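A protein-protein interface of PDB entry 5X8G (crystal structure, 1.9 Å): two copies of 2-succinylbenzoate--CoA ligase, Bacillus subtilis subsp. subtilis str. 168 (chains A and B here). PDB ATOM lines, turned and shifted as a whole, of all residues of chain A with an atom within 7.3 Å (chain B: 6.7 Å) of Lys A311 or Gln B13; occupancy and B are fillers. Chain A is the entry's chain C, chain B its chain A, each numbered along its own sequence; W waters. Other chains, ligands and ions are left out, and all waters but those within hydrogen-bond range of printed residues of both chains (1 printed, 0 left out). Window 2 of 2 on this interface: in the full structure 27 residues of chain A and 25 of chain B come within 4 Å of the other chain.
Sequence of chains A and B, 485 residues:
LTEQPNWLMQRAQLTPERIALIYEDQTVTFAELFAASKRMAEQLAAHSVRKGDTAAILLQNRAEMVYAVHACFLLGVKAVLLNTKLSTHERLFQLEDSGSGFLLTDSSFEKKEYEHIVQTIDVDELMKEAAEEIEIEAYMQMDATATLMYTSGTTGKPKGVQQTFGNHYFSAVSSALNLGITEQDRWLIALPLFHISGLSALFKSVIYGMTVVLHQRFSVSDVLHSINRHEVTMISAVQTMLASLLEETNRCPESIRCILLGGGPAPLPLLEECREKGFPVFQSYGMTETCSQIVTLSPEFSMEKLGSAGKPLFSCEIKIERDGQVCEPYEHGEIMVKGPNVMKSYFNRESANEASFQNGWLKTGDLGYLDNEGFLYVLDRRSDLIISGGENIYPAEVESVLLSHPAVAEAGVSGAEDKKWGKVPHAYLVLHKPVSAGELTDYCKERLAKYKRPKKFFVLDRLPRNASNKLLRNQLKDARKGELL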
ATOM      1  N   ASN A 178     -17.293  32.432  24.325  1.00  0.00           N
ATOM      2  CA  ASN A 178     -16.349  31.975  23.308  1.00  0.00           C
ATOM      3  C   ASN A 178     -16.643  32.601  21.952  1.00  0.00           C
ATOM      4  O   ASN A 178     -15.730  33.083  21.272  1.00  0.00           O
ATOM      5  CB  ASN A 178     -16.382  30.443  23.199  1.00  0.00           C
ATOM      6  CG  ASN A 178     -15.406  29.898  22.143  1.00  0.00           C
ATOM      7  OD1 ASN A 178     -15.796  29.154  21.238  1.00  0.00           O
ATOM      8  ND2 ASN A 178     -14.140  30.264  22.263  1.00  0.00           N
ATOM      9  N   GLN A 283     -14.599  23.675  14.955  1.00  0.00           N
ATOM     10  CA  GLN A 283     -14.621  22.303  15.438  1.00  0.00           C
ATOM     11  C   GLN A 283     -14.752  22.313  16.957  1.00  0.00           C
ATOM     12  O   GLN A 283     -14.295  23.237  17.639  1.00  0.00           O
ATOM     13  CB  GLN A 283     -13.354  21.553  14.996  1.00  0.00           C
ATOM     14  CG  GLN A 283     -13.187  20.148  15.578  1.00  0.00           C
ATOM     15  CD  GLN A 283     -14.037  19.099  14.872  1.00  0.00           C
ATOM     16  OE1 GLN A 283     -13.575  18.418  13.950  1.00  0.00           O
ATOM     17  NE2 GLN A 283     -15.294  18.966  15.303  1.00  0.00           N
ATOM     18  N   ILE A 294     -17.562  21.315  25.154  1.00  0.00           N
ATOM     19  CA  ILE A 294     -16.776  21.707  26.320  1.00  0.00           C
ATOM     20  C   ILE A 294     -15.392  22.169  25.870  1.00  0.00           C
ATOM     21  O   ILE A 294     -14.680  22.833  26.630  1.00  0.00           O
ATOM     22  CB  ILE A 294     -16.700  20.570  27.367  1.00  0.00           C
ATOM     23  CG1 ILE A 294     -16.050  21.064  28.670  1.00  0.00           C
ATOM     24  CG2 ILE A 294     -15.983  19.310  26.800  1.00  0.00           C
ATOM     25  CD1 ILE A 294     -16.396  20.210  29.886  1.00  0.00           C
ATOM     26  N   VAL A 295     -15.031  21.882  24.617  1.00  0.00           N
ATOM     27  CA  VAL A 295     -13.785  22.342  24.000  1.00  0.00           C
ATOM     28  C   VAL A 295     -14.092  22.748  22.556  1.00  0.00           C
ATOM     29  O   VAL A 295     -14.752  21.993  21.836  1.00  0.00           O
ATOM     30  CB  VAL A 295     -12.703  21.232  24.057  1.00  0.00           C
ATOM     31  CG1 VAL A 295     -11.415  21.656  23.364  1.00  0.00           C
ATOM     32  CG2 VAL A 295     -12.396  20.830  25.509  1.00  0.00           C
ATOM     33  N   THR A 296     -13.610  23.929  22.116  1.00  0.00           N
ATOM     34  CA  THR A 296     -13.904  24.432  20.772  1.00  0.00           C
ATOM     35  C   THR A 296     -12.678  25.094  20.139  1.00  0.00           C
ATOM     36  O   THR A 296     -11.858  25.706  20.830  1.00  0.00           O
ATOM     37  CB  THR A 296     -15.096  25.433  20.815  1.00  0.00           C
ATOM     38  OG1 THR A 296     -16.194  24.843  21.527  1.00  0.00           O
ATOM     39  CG2 THR A 296     -15.574  25.790  19.421  1.00  0.00           C
ATOM     40  N   LEU A 297     -12.568  24.978  18.809  1.00  0.00           N
ATOM     41  CA  LEU A 297     -11.407  25.429  18.033  1.00  0.00           C
ATOM     42  C   LEU A 297     -11.809  26.504  17.033  1.00  0.00           C
ATOM     43  O   LEU A 297     -12.621  26.243  16.138  1.00  0.00           O
ATOM     44  CB  LEU A 297     -10.764  24.264  17.266  1.00  0.00           C
ATOM     45  CG  LEU A 297      -9.572  24.629  16.362  1.00  0.00           C
ATOM     46  CD1 LEU A 297      -8.274  24.806  17.177  1.00  0.00           C
ATOM     47  CD2 LEU A 297      -9.365  23.632  15.202  1.00  0.00           C
ATOM     48  N   SER A 298     -11.182  27.685  17.128  1.00  0.00           N
ATOM     49  CA  SER A 298     -11.499  28.805  16.240  1.00  0.00           C
ATOM     50  C   SER A 298     -10.928  28.595  14.831  1.00  0.00           C
ATOM     51  O   SER A 298      -9.891  27.945  14.662  1.00  0.00           O
ATOM     52  CB  SER A 298     -10.949  30.110  16.815  1.00  0.00           C
ATOM     53  OG  SER A 298     -11.515  30.407  18.086  1.00  0.00           O
ATOM     54  N   PHE A 301      -7.113  29.129  14.067  1.00  0.00           N
ATOM     55  CA  PHE A 301      -6.145  28.099  14.413  1.00  0.00           C
ATOM     56  C   PHE A 301      -6.375  26.805  13.649  1.00  0.00           C
ATOM     57  O   PHE A 301      -5.592  25.862  13.805  1.00  0.00           O
ATOM     58  CB  PHE A 301      -6.184  27.821  15.921  1.00  0.00           C
ATOM     59  CG  PHE A 301      -5.923  29.032  16.778  1.00  0.00           C
ATOM     60  CD1 PHE A 301      -4.649  29.573  16.867  1.00  0.00           C
ATOM     61  CD2 PHE A 301      -6.945  29.610  17.518  1.00  0.00           C
ATOM     62  CE1 PHE A 301      -4.405  30.680  17.661  1.00  0.00           C
ATOM     63  CE2 PHE A 301      -6.702  30.714  18.315  1.00  0.00           C
ATOM     64  CZ  PHE A 301      -5.432  31.250  18.385  1.00  0.00           C
ATOM     65  N   SER A 308      -7.316  19.362  15.672  1.00  0.00           N
ATOM     66  CA  SER A 308      -7.564  19.645  17.079  1.00  0.00           C
ATOM     67  C   SER A 308      -9.004  20.096  17.299  1.00  0.00           C
ATOM     68  O   SER A 308      -9.633  20.692  16.420  1.00  0.00           O
ATOM     69  CB  SER A 308      -6.601  20.723  17.587  1.00  0.00           C
ATOM     70  OG  SER A 308      -6.993  21.208  18.863  1.00  0.00           O
ATOM     71  N   ALA A 309      -9.522  19.804  18.486  1.00  0.00           N
ATOM     72  CA  ALA A 309     -10.849  20.246  18.896  1.00  0.00           C
ATOM     73  C   ALA A 309     -10.813  21.557  19.662  1.00  0.00           C
ATOM     74  O   ALA A 309     -11.872  22.068  20.043  1.00  0.00           O
ATOM     75  CB  ALA A 309     -11.530  19.176  19.760  1.00  0.00           C
ATOM     76  N   GLY A 310      -9.624  22.095  19.915  1.00  0.00           N
ATOM     77  CA  GLY A 310      -9.493  23.409  20.506  1.00  0.00           C
ATOM     78  C   GLY A 310      -9.081  23.441  21.959  1.00  0.00           C
ATOM     79  O   GLY A 310      -8.314  22.591  22.436  1.00  0.00           O
ATOM     80  N   LYS A 311      -9.611  24.425  22.674  1.00  0.00           N
ATOM     81  CA  LYS A 311      -9.321  24.687  24.074  1.00  0.00           C
ATOM     82  C   LYS A 311     -10.608  24.667  24.887  1.00  0.00           C
ATOM     83  O   LYS A 311     -11.690  24.911  24.344  1.00  0.00           O
ATOM     84  CB  LYS A 311      -8.634  26.052  24.227  1.00  0.00           C
ATOM     85  CG  LYS A 311      -7.440  26.227  23.305  1.00  0.00           C
ATOM     86  CD  LYS A 311      -6.145  26.030  24.064  1.00  0.00           C
ATOM     87  CE  LYS A 311      -5.731  27.308  24.752  1.00  0.00           C
ATOM     88  NZ  LYS A 311      -4.303  27.274  25.176  1.00  0.00           N
ATOM     89  N   PRO A 312     -10.537  24.382  26.186  1.00  0.00           N
ATOM     90  CA  PRO A 312     -11.768  24.335  26.986  1.00  0.00           C
ATOM     91  C   PRO A 312     -12.470  25.694  27.043  1.00  0.00           C
ATOM     92  O   PRO A 312     -11.829  26.749  27.063  1.00  0.00           O
ATOM     93  CB  PRO A 312     -11.273  23.890  28.362  1.00  0.00           C
ATOM     94  CG  PRO A 312      -9.812  24.300  28.402  1.00  0.00           C
ATOM     95  CD  PRO A 312      -9.328  24.102  26.995  1.00  0.00           C
ATOM     96  N   LEU A 313     -13.804  25.652  27.058  1.00  0.00           N
ATOM     97  CA  LEU A 313     -14.590  26.862  27.247  1.00  0.00           C
ATOM     98  C   LEU A 313     -14.313  27.452  28.628  1.00  0.00           C
ATOM     99  O   LEU A 313     -13.816  26.774  29.538  1.00  0.00           O
ATOM    100  CB  LEU A 313     -16.093  26.569  27.086  1.00  0.00           C
ATOM    101  CG  LEU A 313     -16.550  26.000  25.736  1.00  0.00           C
ATOM    102  CD1 LEU A 313     -18.042  25.730  25.742  1.00  0.00           C
ATOM    103  CD2 LEU A 313     -16.191  26.927  24.582  1.00  0.00           C
ATOM    104  N   PHE A 314     -14.621  28.735  28.769  1.00  0.00           N
ATOM    105  CA  PHE A 314     -14.401  29.420  30.034  1.00  0.00           C
ATOM    106  C   PHE A 314     -15.223  28.731  31.109  1.00  0.00           C
ATOM    107  O   PHE A 314     -16.338  28.261  30.850  1.00  0.00           O
ATOM    108  CB  PHE A 314     -14.776  30.900  29.903  1.00  0.00           C
ATOM    109  CG  PHE A 314     -14.029  31.794  30.833  1.00  0.00           C
ATOM    110  CD1 PHE A 314     -12.729  32.154  30.537  1.00  0.00           C
ATOM    111  CD2 PHE A 314     -14.579  32.200  32.032  1.00  0.00           C
ATOM    112  CE1 PHE A 314     -12.007  32.955  31.380  1.00  0.00           C
ATOM    113  CE2 PHE A 314     -13.850  33.015  32.884  1.00  0.00           C
ATOM    114  CZ  PHE A 314     -12.574  33.381  32.554  1.00  0.00           C
ATOM    115  N   CYS A 316     -14.527  25.879  32.250  1.00  0.00           N
ATOM    116  CA  CYS A 316     -14.351  24.445  32.061  1.00  0.00           C
ATOM    117  C   CYS A 316     -12.872  24.085  32.033  1.00  0.00           C
ATOM    118  O   CYS A 316     -11.998  24.937  31.883  1.00  0.00           O
ATOM    119  CB  CYS A 316     -15.005  23.977  30.765  1.00  0.00           C
ATOM    120  SG  CYS A 316     -16.708  24.515  30.586  1.00  0.00           S
ATOM    121  N   GLU A 317     -12.607  22.786  32.145  1.00  0.00           N
ATOM    122  CA  GLU A 317     -11.252  22.280  32.311  1.00  0.00           C
ATOM    123  C   GLU A 317     -11.145  20.896  31.685  1.00  0.00           C
ATOM    124  O   GLU A 317     -12.120  20.142  31.644  1.00  0.00           O
ATOM    125  CB  GLU A 317     -10.852  22.173  33.784  1.00  0.00           C
ATOM    126  CG  GLU A 317     -10.982  23.412  34.635  1.00  0.00           C
ATOM    127  CD  GLU A 317     -10.817  23.083  36.108  1.00  0.00           C
ATOM    128  OE1 GLU A 317     -11.845  23.017  36.827  1.00  0.00           O
ATOM    129  OE2 GLU A 317      -9.664  22.862  36.526  1.00  0.00           O
ATOM    130  N   ILE A 318      -9.931  20.556  31.241  1.00  0.00           N
ATOM    131  CA  ILE A 318      -9.639  19.268  30.627  1.00  0.00           C
ATOM    132  C   ILE A 318      -8.241  18.833  31.050  1.00  0.00           C
ATOM    133  O   ILE A 318      -7.348  19.662  31.244  1.00  0.00           O
ATOM    134  CB  ILE A 318      -9.739  19.326  29.086  1.00  0.00           C
ATOM    135  CG1 ILE A 318      -9.487  17.945  28.484  1.00  0.00           C
ATOM    136  CG2 ILE A 318      -8.761  20.357  28.512  1.00  0.00           C
ATOM    137  CD1 ILE A 318      -9.131  17.987  27.046  1.00  0.00           C
ATOM    138  N   LEU A 370      -2.838  16.575  24.774  1.00  0.00           N
ATOM    139  CA  LEU A 370      -2.720  18.018  24.635  1.00  0.00           C
ATOM    140  C   LEU A 370      -1.386  18.353  23.996  1.00  0.00           C
ATOM    141  O   LEU A 370      -0.370  17.715  24.298  1.00  0.00           O
ATOM    142  CB  LEU A 370      -2.828  18.725  25.988  1.00  0.00           C
ATOM    143  CG  LEU A 370      -4.143  18.437  26.713  1.00  0.00           C
ATOM    144  CD1 LEU A 370      -4.047  18.841  28.173  1.00  0.00           C
ATOM    145  CD2 LEU A 370      -5.271  19.138  26.031  1.00  0.00           C
ATOM    146  N   ASP A 371      -1.382  19.345  23.110  1.00  0.00           N
ATOM    147  CA  ASP A 371      -0.095  19.787  22.607  1.00  0.00           C
ATOM    148  C   ASP A 371       0.520  20.765  23.612  1.00  0.00           C
ATOM    149  O   ASP A 371      -0.023  21.006  24.696  1.00  0.00           O
ATOM    150  CB  ASP A 371      -0.214  20.345  21.183  1.00  0.00           C
ATOM    151  CG  ASP A 371      -0.911  21.706  21.100  1.00  0.00           C
ATOM    152  OD1 ASP A 371      -1.171  22.348  22.138  1.00  0.00           O
ATOM    153  OD2 ASP A 371      -1.170  22.146  19.952  1.00  0.00           O
ATOM    154  N   ASN A 372       1.678  21.324  23.272  1.00  0.00           N
ATOM    155  CA  ASN A 372       2.394  22.117  24.266  1.00  0.00           C
ATOM    156  C   ASN A 372       1.799  23.504  24.468  1.00  0.00           C
ATOM    157  O   ASN A 372       2.315  24.249  25.304  1.00  0.00           O
ATOM    158  CB  ASN A 372       3.888  22.224  23.917  1.00  0.00           C
ATOM    159  CG  ASN A 372       4.143  22.844  22.554  1.00  0.00           C
ATOM    160  OD1 ASN A 372       3.247  23.395  21.923  1.00  0.00           O
ATOM    161  ND2 ASN A 372       5.390  22.756  22.099  1.00  0.00           N
ATOM    162  N   GLU A 373       0.740  23.865  23.736  1.00  0.00           N
ATOM    163  CA  GLU A 373      -0.021  25.078  24.018  1.00  0.00           C
ATOM    164  C   GLU A 373      -1.382  24.762  24.611  1.00  0.00           C
ATOM    165  O   GLU A 373      -2.214  25.668  24.782  1.00  0.00           O
ATOM    166  CB  GLU A 373      -0.170  25.922  22.755  1.00  0.00           C
ATOM    167  CG  GLU A 373       1.164  26.326  22.147  1.00  0.00           C
ATOM    168  CD  GLU A 373       1.000  27.160  20.899  1.00  0.00           C
ATOM    169  OE1 GLU A 373       0.247  26.734  20.000  1.00  0.00           O
ATOM    170  OE2 GLU A 373       1.629  28.231  20.804  1.00  0.00           O
ATOM    171  N   GLY A 374      -1.629  23.496  24.933  1.00  0.00           N
ATOM    172  CA  GLY A 374      -2.861  23.094  25.569  1.00  0.00           C
ATOM    173  C   GLY A 374      -4.016  22.810  24.635  1.00  0.00           C
ATOM    174  O   GLY A 374      -5.142  22.650  25.110  1.00  0.00           O
ATOM    175  N   PHE A 375      -3.782  22.736  23.327  1.00  0.00           N
ATOM    176  CA  PHE A 375      -4.847  22.354  22.402  1.00  0.00           C
ATOM    177  C   PHE A 375      -5.106  20.854  22.473  1.00  0.00           C
ATOM    178  O   PHE A 375      -4.172  20.047  22.554  1.00  0.00           O
ATOM    179  CB  PHE A 375      -4.488  22.752  20.969  1.00  0.00           C
ATOM    180  CG  PHE A 375      -4.579  24.226  20.711  1.00  0.00           C
ATOM    181  CD1 PHE A 375      -3.575  25.080  21.133  1.00  0.00           C
ATOM    182  CD2 PHE A 375      -5.670  24.760  20.045  1.00  0.00           C
ATOM    183  CE1 PHE A 375      -3.647  26.442  20.894  1.00  0.00           C
ATOM    184  CE2 PHE A 375      -5.750  26.125  19.807  1.00  0.00           C
ATOM    185  CZ  PHE A 375      -4.744  26.966  20.244  1.00  0.00           C
ATOM    186  N   LEU A 376      -6.385  20.480  22.417  1.00  0.00           N
ATOM    187  CA  LEU A 376      -6.798  19.090  22.542  1.00  0.00           C
ATOM    188  C   LEU A 376      -6.819  18.402  21.181  1.00  0.00           C
ATOM    189  O   LEU A 376      -7.338  18.957  20.207  1.00  0.00           O
ATOM    190  CB  LEU A 376      -8.182  18.998  23.191  1.00  0.00           C
ATOM    191  CG  LEU A 376      -8.773  17.584  23.212  1.00  0.00           C
ATOM    192  CD1 LEU A 376      -7.923  16.622  24.087  1.00  0.00           C
ATOM    193  CD2 LEU A 376     -10.220  17.606  23.686  1.00  0.00           C
ATOM    194  N   PRO B   5     -12.062  27.913  37.782  1.00  0.00           N
ATOM    195  CA  PRO B   5     -10.653  28.293  37.609  1.00  0.00           C
ATOM    196  C   PRO B   5     -10.498  29.798  37.742  1.00  0.00           C
ATOM    197  O   PRO B   5     -11.357  30.568  37.308  1.00  0.00           O
ATOM    198  CB  PRO B   5     -10.321  27.824  36.188  1.00  0.00           C
ATOM    199  CG  PRO B   5     -11.337  26.741  35.894  1.00  0.00           C
ATOM    200  CD  PRO B   5     -12.595  27.180  36.616  1.00  0.00           C
ATOM    201  N   ASN B   6      -9.397  30.213  38.366  1.00  0.00           N
ATOM    202  CA  ASN B   6      -9.121  31.633  38.484  1.00  0.00           C
ATOM    203  C   ASN B   6      -9.235  32.286  37.114  1.00  0.00           C
ATOM    204  O   ASN B   6      -8.666  31.790  36.133  1.00  0.00           O
ATOM    205  CB  ASN B   6      -7.721  31.830  39.082  1.00  0.00           C
ATOM    206  CG  ASN B   6      -7.263  33.253  39.011  1.00  0.00           C
ATOM    207  OD1 ASN B   6      -6.876  33.732  37.945  1.00  0.00           O
ATOM    208  ND2 ASN B   6      -7.256  33.934  40.156  1.00  0.00           N
ATOM    209  N   LEU B   8      -8.206  35.124  35.741  1.00  0.00           N
ATOM    210  CA  LEU B   8      -7.015  35.639  35.076  1.00  0.00           C
ATOM    211  C   LEU B   8      -6.169  34.496  34.542  1.00  0.00           C
ATOM    212  O   LEU B   8      -5.669  34.552  33.411  1.00  0.00           O
ATOM    213  CB  LEU B   8      -6.195  36.495  36.043  1.00  0.00           C
ATOM    214  CG  LEU B   8      -4.844  36.989  35.519  1.00  0.00           C
ATOM    215  CD1 LEU B   8      -5.000  37.765  34.196  1.00  0.00           C
ATOM    216  CD2 LEU B   8      -4.195  37.860  36.585  1.00  0.00           C
ATOM    217  N   MET B   9      -6.041  33.441  35.331  1.00  0.00           N
ATOM    218  CA  MET B   9      -5.226  32.304  34.926  1.00  0.00           C
ATOM    219  C   MET B   9      -5.811  31.635  33.683  1.00  0.00           C
ATOM    220  O   MET B   9      -5.098  31.379  32.707  1.00  0.00           O
ATOM    221  CB  MET B   9      -5.146  31.310  36.076  1.00  0.00           C
ATOM    222  CG  MET B   9      -4.496  29.974  35.694  1.00  0.00           C
ATOM    223  SD  MET B   9      -4.433  28.843  37.073  1.00  0.00           S
ATOM    224  CE  MET B   9      -5.909  27.860  36.798  1.00  0.00           C
ATOM    225  N   GLN B  10      -7.123  31.376  33.679  1.00  0.00           N
ATOM    226  CA  GLN B  10      -7.726  30.753  32.503  1.00  0.00           C
ATOM    227  C   GLN B  10      -7.656  31.668  31.290  1.00  0.00           C
ATOM    228  O   GLN B  10      -7.331  31.214  30.186  1.00  0.00           O
ATOM    229  CB  GLN B  10      -9.174  30.336  32.763  1.00  0.00           C
ATOM    230  CG  GLN B  10      -9.710  29.549  31.556  1.00  0.00           C
ATOM    231  CD  GLN B  10     -10.991  28.772  31.809  1.00  0.00           C
ATOM    232  OE1 GLN B  10     -11.749  29.069  32.726  1.00  0.00           O
ATOM    233  NE2 GLN B  10     -11.208  27.723  31.010  1.00  0.00           N
ATOM    234  N   ARG B  11      -7.944  32.960  31.470  1.00  0.00           N
ATOM    235  CA  ARG B  11      -7.890  33.889  30.345  1.00  0.00           C
ATOM    236  C   ARG B  11      -6.491  33.943  29.732  1.00  0.00           C
ATOM    237  O   ARG B  11      -6.339  33.957  28.503  1.00  0.00           O
ATOM    238  CB  ARG B  11      -8.340  35.279  30.800  1.00  0.00           C
ATOM    239  CG  ARG B  11      -8.296  36.339  29.720  1.00  0.00           C
ATOM    240  CD  ARG B  11      -8.957  35.864  28.423  1.00  0.00           C
ATOM    241  NE  ARG B  11     -10.370  35.526  28.581  1.00  0.00           N
ATOM    242  CZ  ARG B  11     -11.084  34.898  27.649  1.00  0.00           C
ATOM    243  NH1 ARG B  11     -12.371  34.643  27.849  1.00  0.00           N
ATOM    244  NH2 ARG B  11     -10.512  34.544  26.503  1.00  0.00           N
ATOM    245  N   ALA B  12      -5.456  33.980  30.572  1.00  0.00           N
ATOM    246  CA  ALA B  12      -4.094  33.934  30.044  1.00  0.00           C
ATOM    247  C   ALA B  12      -3.809  32.612  29.339  1.00  0.00           C
ATOM    248  O   ALA B  12      -3.045  32.580  28.366  1.00  0.00           O
ATOM    249  CB  ALA B  12      -3.089  34.175  31.169  1.00  0.00           C
ATOM    250  N   GLN B  13      -4.362  31.530  29.830  1.00  0.00           N
ATOM    251  CA  GLN B  13      -4.265  30.242  29.147  1.00  0.00           C
ATOM    252  C   GLN B  13      -4.931  30.230  27.774  1.00  0.00           C
ATOM    253  O   GLN B  13      -4.401  29.639  26.861  1.00  0.00           O
ATOM    254  CB  GLN B  13      -4.794  29.090  29.988  1.00  0.00           C
ATOM    255  CG  GLN B  13      -3.927  28.740  31.169  1.00  0.00           C
ATOM    256  CD  GLN B  13      -4.609  27.876  32.205  1.00  0.00           C
ATOM    257  OE1 GLN B  13      -4.033  27.569  33.217  1.00  0.00           O
ATOM    258  NE2 GLN B  13      -5.809  27.498  31.958  1.00  0.00           N
ATOM    259  N   LEU B  14      -6.088  30.892  27.655  1.00  0.00           N
ATOM    260  CA  LEU B  14      -6.907  30.826  26.449  1.00  0.00           C
ATOM    261  C   LEU B  14      -6.438  31.802  25.378  1.00  0.00           C
ATOM    262  O   LEU B  14      -6.296  31.427  24.212  1.00  0.00           O
ATOM    263  CB  LEU B  14      -8.377  31.096  26.792  1.00  0.00           C
ATOM    264  CG  LEU B  14      -9.076  30.010  27.611  1.00  0.00           C
ATOM    265  CD1 LEU B  14     -10.568  30.335  27.763  1.00  0.00           C
ATOM    266  CD2 LEU B  14      -8.846  28.635  26.970  1.00  0.00           C
ATOM    267  N   THR B  15      -6.245  33.068  25.737  1.00  0.00           N
ATOM    268  CA  THR B  15      -5.885  34.116  24.784  1.00  0.00           C
ATOM    269  C   THR B  15      -4.755  34.942  25.375  1.00  0.00           C
ATOM    270  O   THR B  15      -4.926  36.122  25.711  1.00  0.00           O
ATOM    271  CB  THR B  15      -7.098  34.982  24.449  1.00  0.00           C
ATOM    272  OG1 THR B  15      -7.583  35.649  25.621  1.00  0.00           O
ATOM    273  CG2 THR B  15      -8.239  34.128  23.856  1.00  0.00           C
ATOM    274  N   PRO B  16      -3.566  34.341  25.497  1.00  0.00           N
ATOM    275  CA  PRO B  16      -2.462  35.020  26.205  1.00  0.00           C
ATOM    276  C   PRO B  16      -2.038  36.334  25.580  1.00  0.00           C
ATOM    277  O   PRO B  16      -1.619  37.248  26.304  1.00  0.00           O
ATOM    278  CB  PRO B  16      -1.298  34.007  26.133  1.00  0.00           C
ATOM    279  CG  PRO B  16      -1.696  33.013  25.104  1.00  0.00           C
ATOM    280  CD  PRO B  16      -3.186  32.981  25.075  1.00  0.00           C
ATOM    281  N   PHE B  30      -2.789  39.624  28.496  1.00  0.00           N
ATOM    282  CA  PHE B  30      -3.246  38.738  29.565  1.00  0.00           C
ATOM    283  C   PHE B  30      -2.125  37.828  30.067  1.00  0.00           C
ATOM    284  O   PHE B  30      -2.067  37.524  31.262  1.00  0.00           O
ATOM    285  CB  PHE B  30      -4.442  37.903  29.089  1.00  0.00           C
ATOM    286  CG  PHE B  30      -5.721  38.690  28.975  1.00  0.00           C
ATOM    287  CD1 PHE B  30      -6.398  39.095  30.119  1.00  0.00           C
ATOM    288  CD2 PHE B  30      -6.235  39.033  27.727  1.00  0.00           C
ATOM    289  CE1 PHE B  30      -7.585  39.820  30.015  1.00  0.00           C
ATOM    290  CE2 PHE B  30      -7.406  39.760  27.612  1.00  0.00           C
ATOM    291  CZ  PHE B  30      -8.077  40.159  28.752  1.00  0.00           C
ATOM    292  N   ALA B  31      -1.225  37.385  29.186  1.00  0.00           N
ATOM    293  CA  ALA B  31      -0.070  36.629  29.664  1.00  0.00           C
ATOM    294  C   ALA B  31       0.790  37.485  30.588  1.00  0.00           C
ATOM    295  O   ALA B  31       1.203  37.041  31.665  1.00  0.00           O
ATOM    296  CB  ALA B  31       0.760  36.108  28.485  1.00  0.00           C
HETATM  297  O   HOH W   1      -9.203  25.329  31.647  1.00  0.00           O
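The backbone carbonyl oxygen (O) of Leu A313 lies within hydrogen-bond range of the side-chain amide nitrogen (NE2) of Gln B10 (3.1 Å).
The backbone carbonyl oxygen (O) of Gln B13 sits at hydrogen-bond distance from the side-chain amino group (NZ) of Lys A311 (2.9 Å).
NE2 of Gln B10 lies within hydrogen-bond range of O of Cys A316, at 3.0 Å.
The side-chain sulfur (SG) of Cys A316 is in hydrogen-bond range of the backbone carbonyl oxygen (O) of Phe A314 (3.8 Å).
O of Glu A373 lies within hydrogen-bond range of NZ of Lys A311.
The side-chain hydroxyl (OG1) of Thr B15 lies close to the guanidinium group (NH2) of Arg B11 (3.3 Å).
The backbone carbonyl oxygen (O) of Lys A311 lies within hydrogen-bond range of the backbone NH (N) of Thr A296 (3.1 Å).
O of Ile A294 lies within hydrogen-bond range of N of Leu A313 (3.0 Å).
Among the printed residues, merely in contact across the chains: Pro A312 with Leu B14 (3.5 Å), Glu A317 with Pro B5 (3.6 Å), Phe A314 with Arg B11 (3.7 Å), Phe A314 with Gln B10 (3.7 Å), Lys A311 with Leu B14 (3.8 Å) and Phe A314 with Leu B14 (3.96 Å).
Of the printed residues of chain B, Cys A316 touches Gln B10 (3.0 Å).
Of the printed residues of chain B, Glu A317 touches Pro B5.
Of the printed residues of chain A, Gln B10 touches Leu A313 (3.1 Å), Phe A314 (3.7 Å) and Cys A316 (3.0 Å).
Of the printed residues of chain B, Pro A312 touches Leu B14 (3.5 Å).
Thr A296 touches none of the printed residues of chain B.
Glu A373 touches none of the printed residues of chain B.
The nearest residue of chain B that does not touch Lys A311 is Pro B16 (5.8 Å).
Hydrophobic or aromatic side chains of chain A within 4 Å of the printed part of chain B: Phe A314.
No position is printed for both chains.
Water W1 lies within hydrogen-bond range of the backbone carbonyl oxygen (O) of Cys A316 (2.8 Å) and the side-chain amide nitrogen (NE2) of Gln B10 (3.2 Å).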
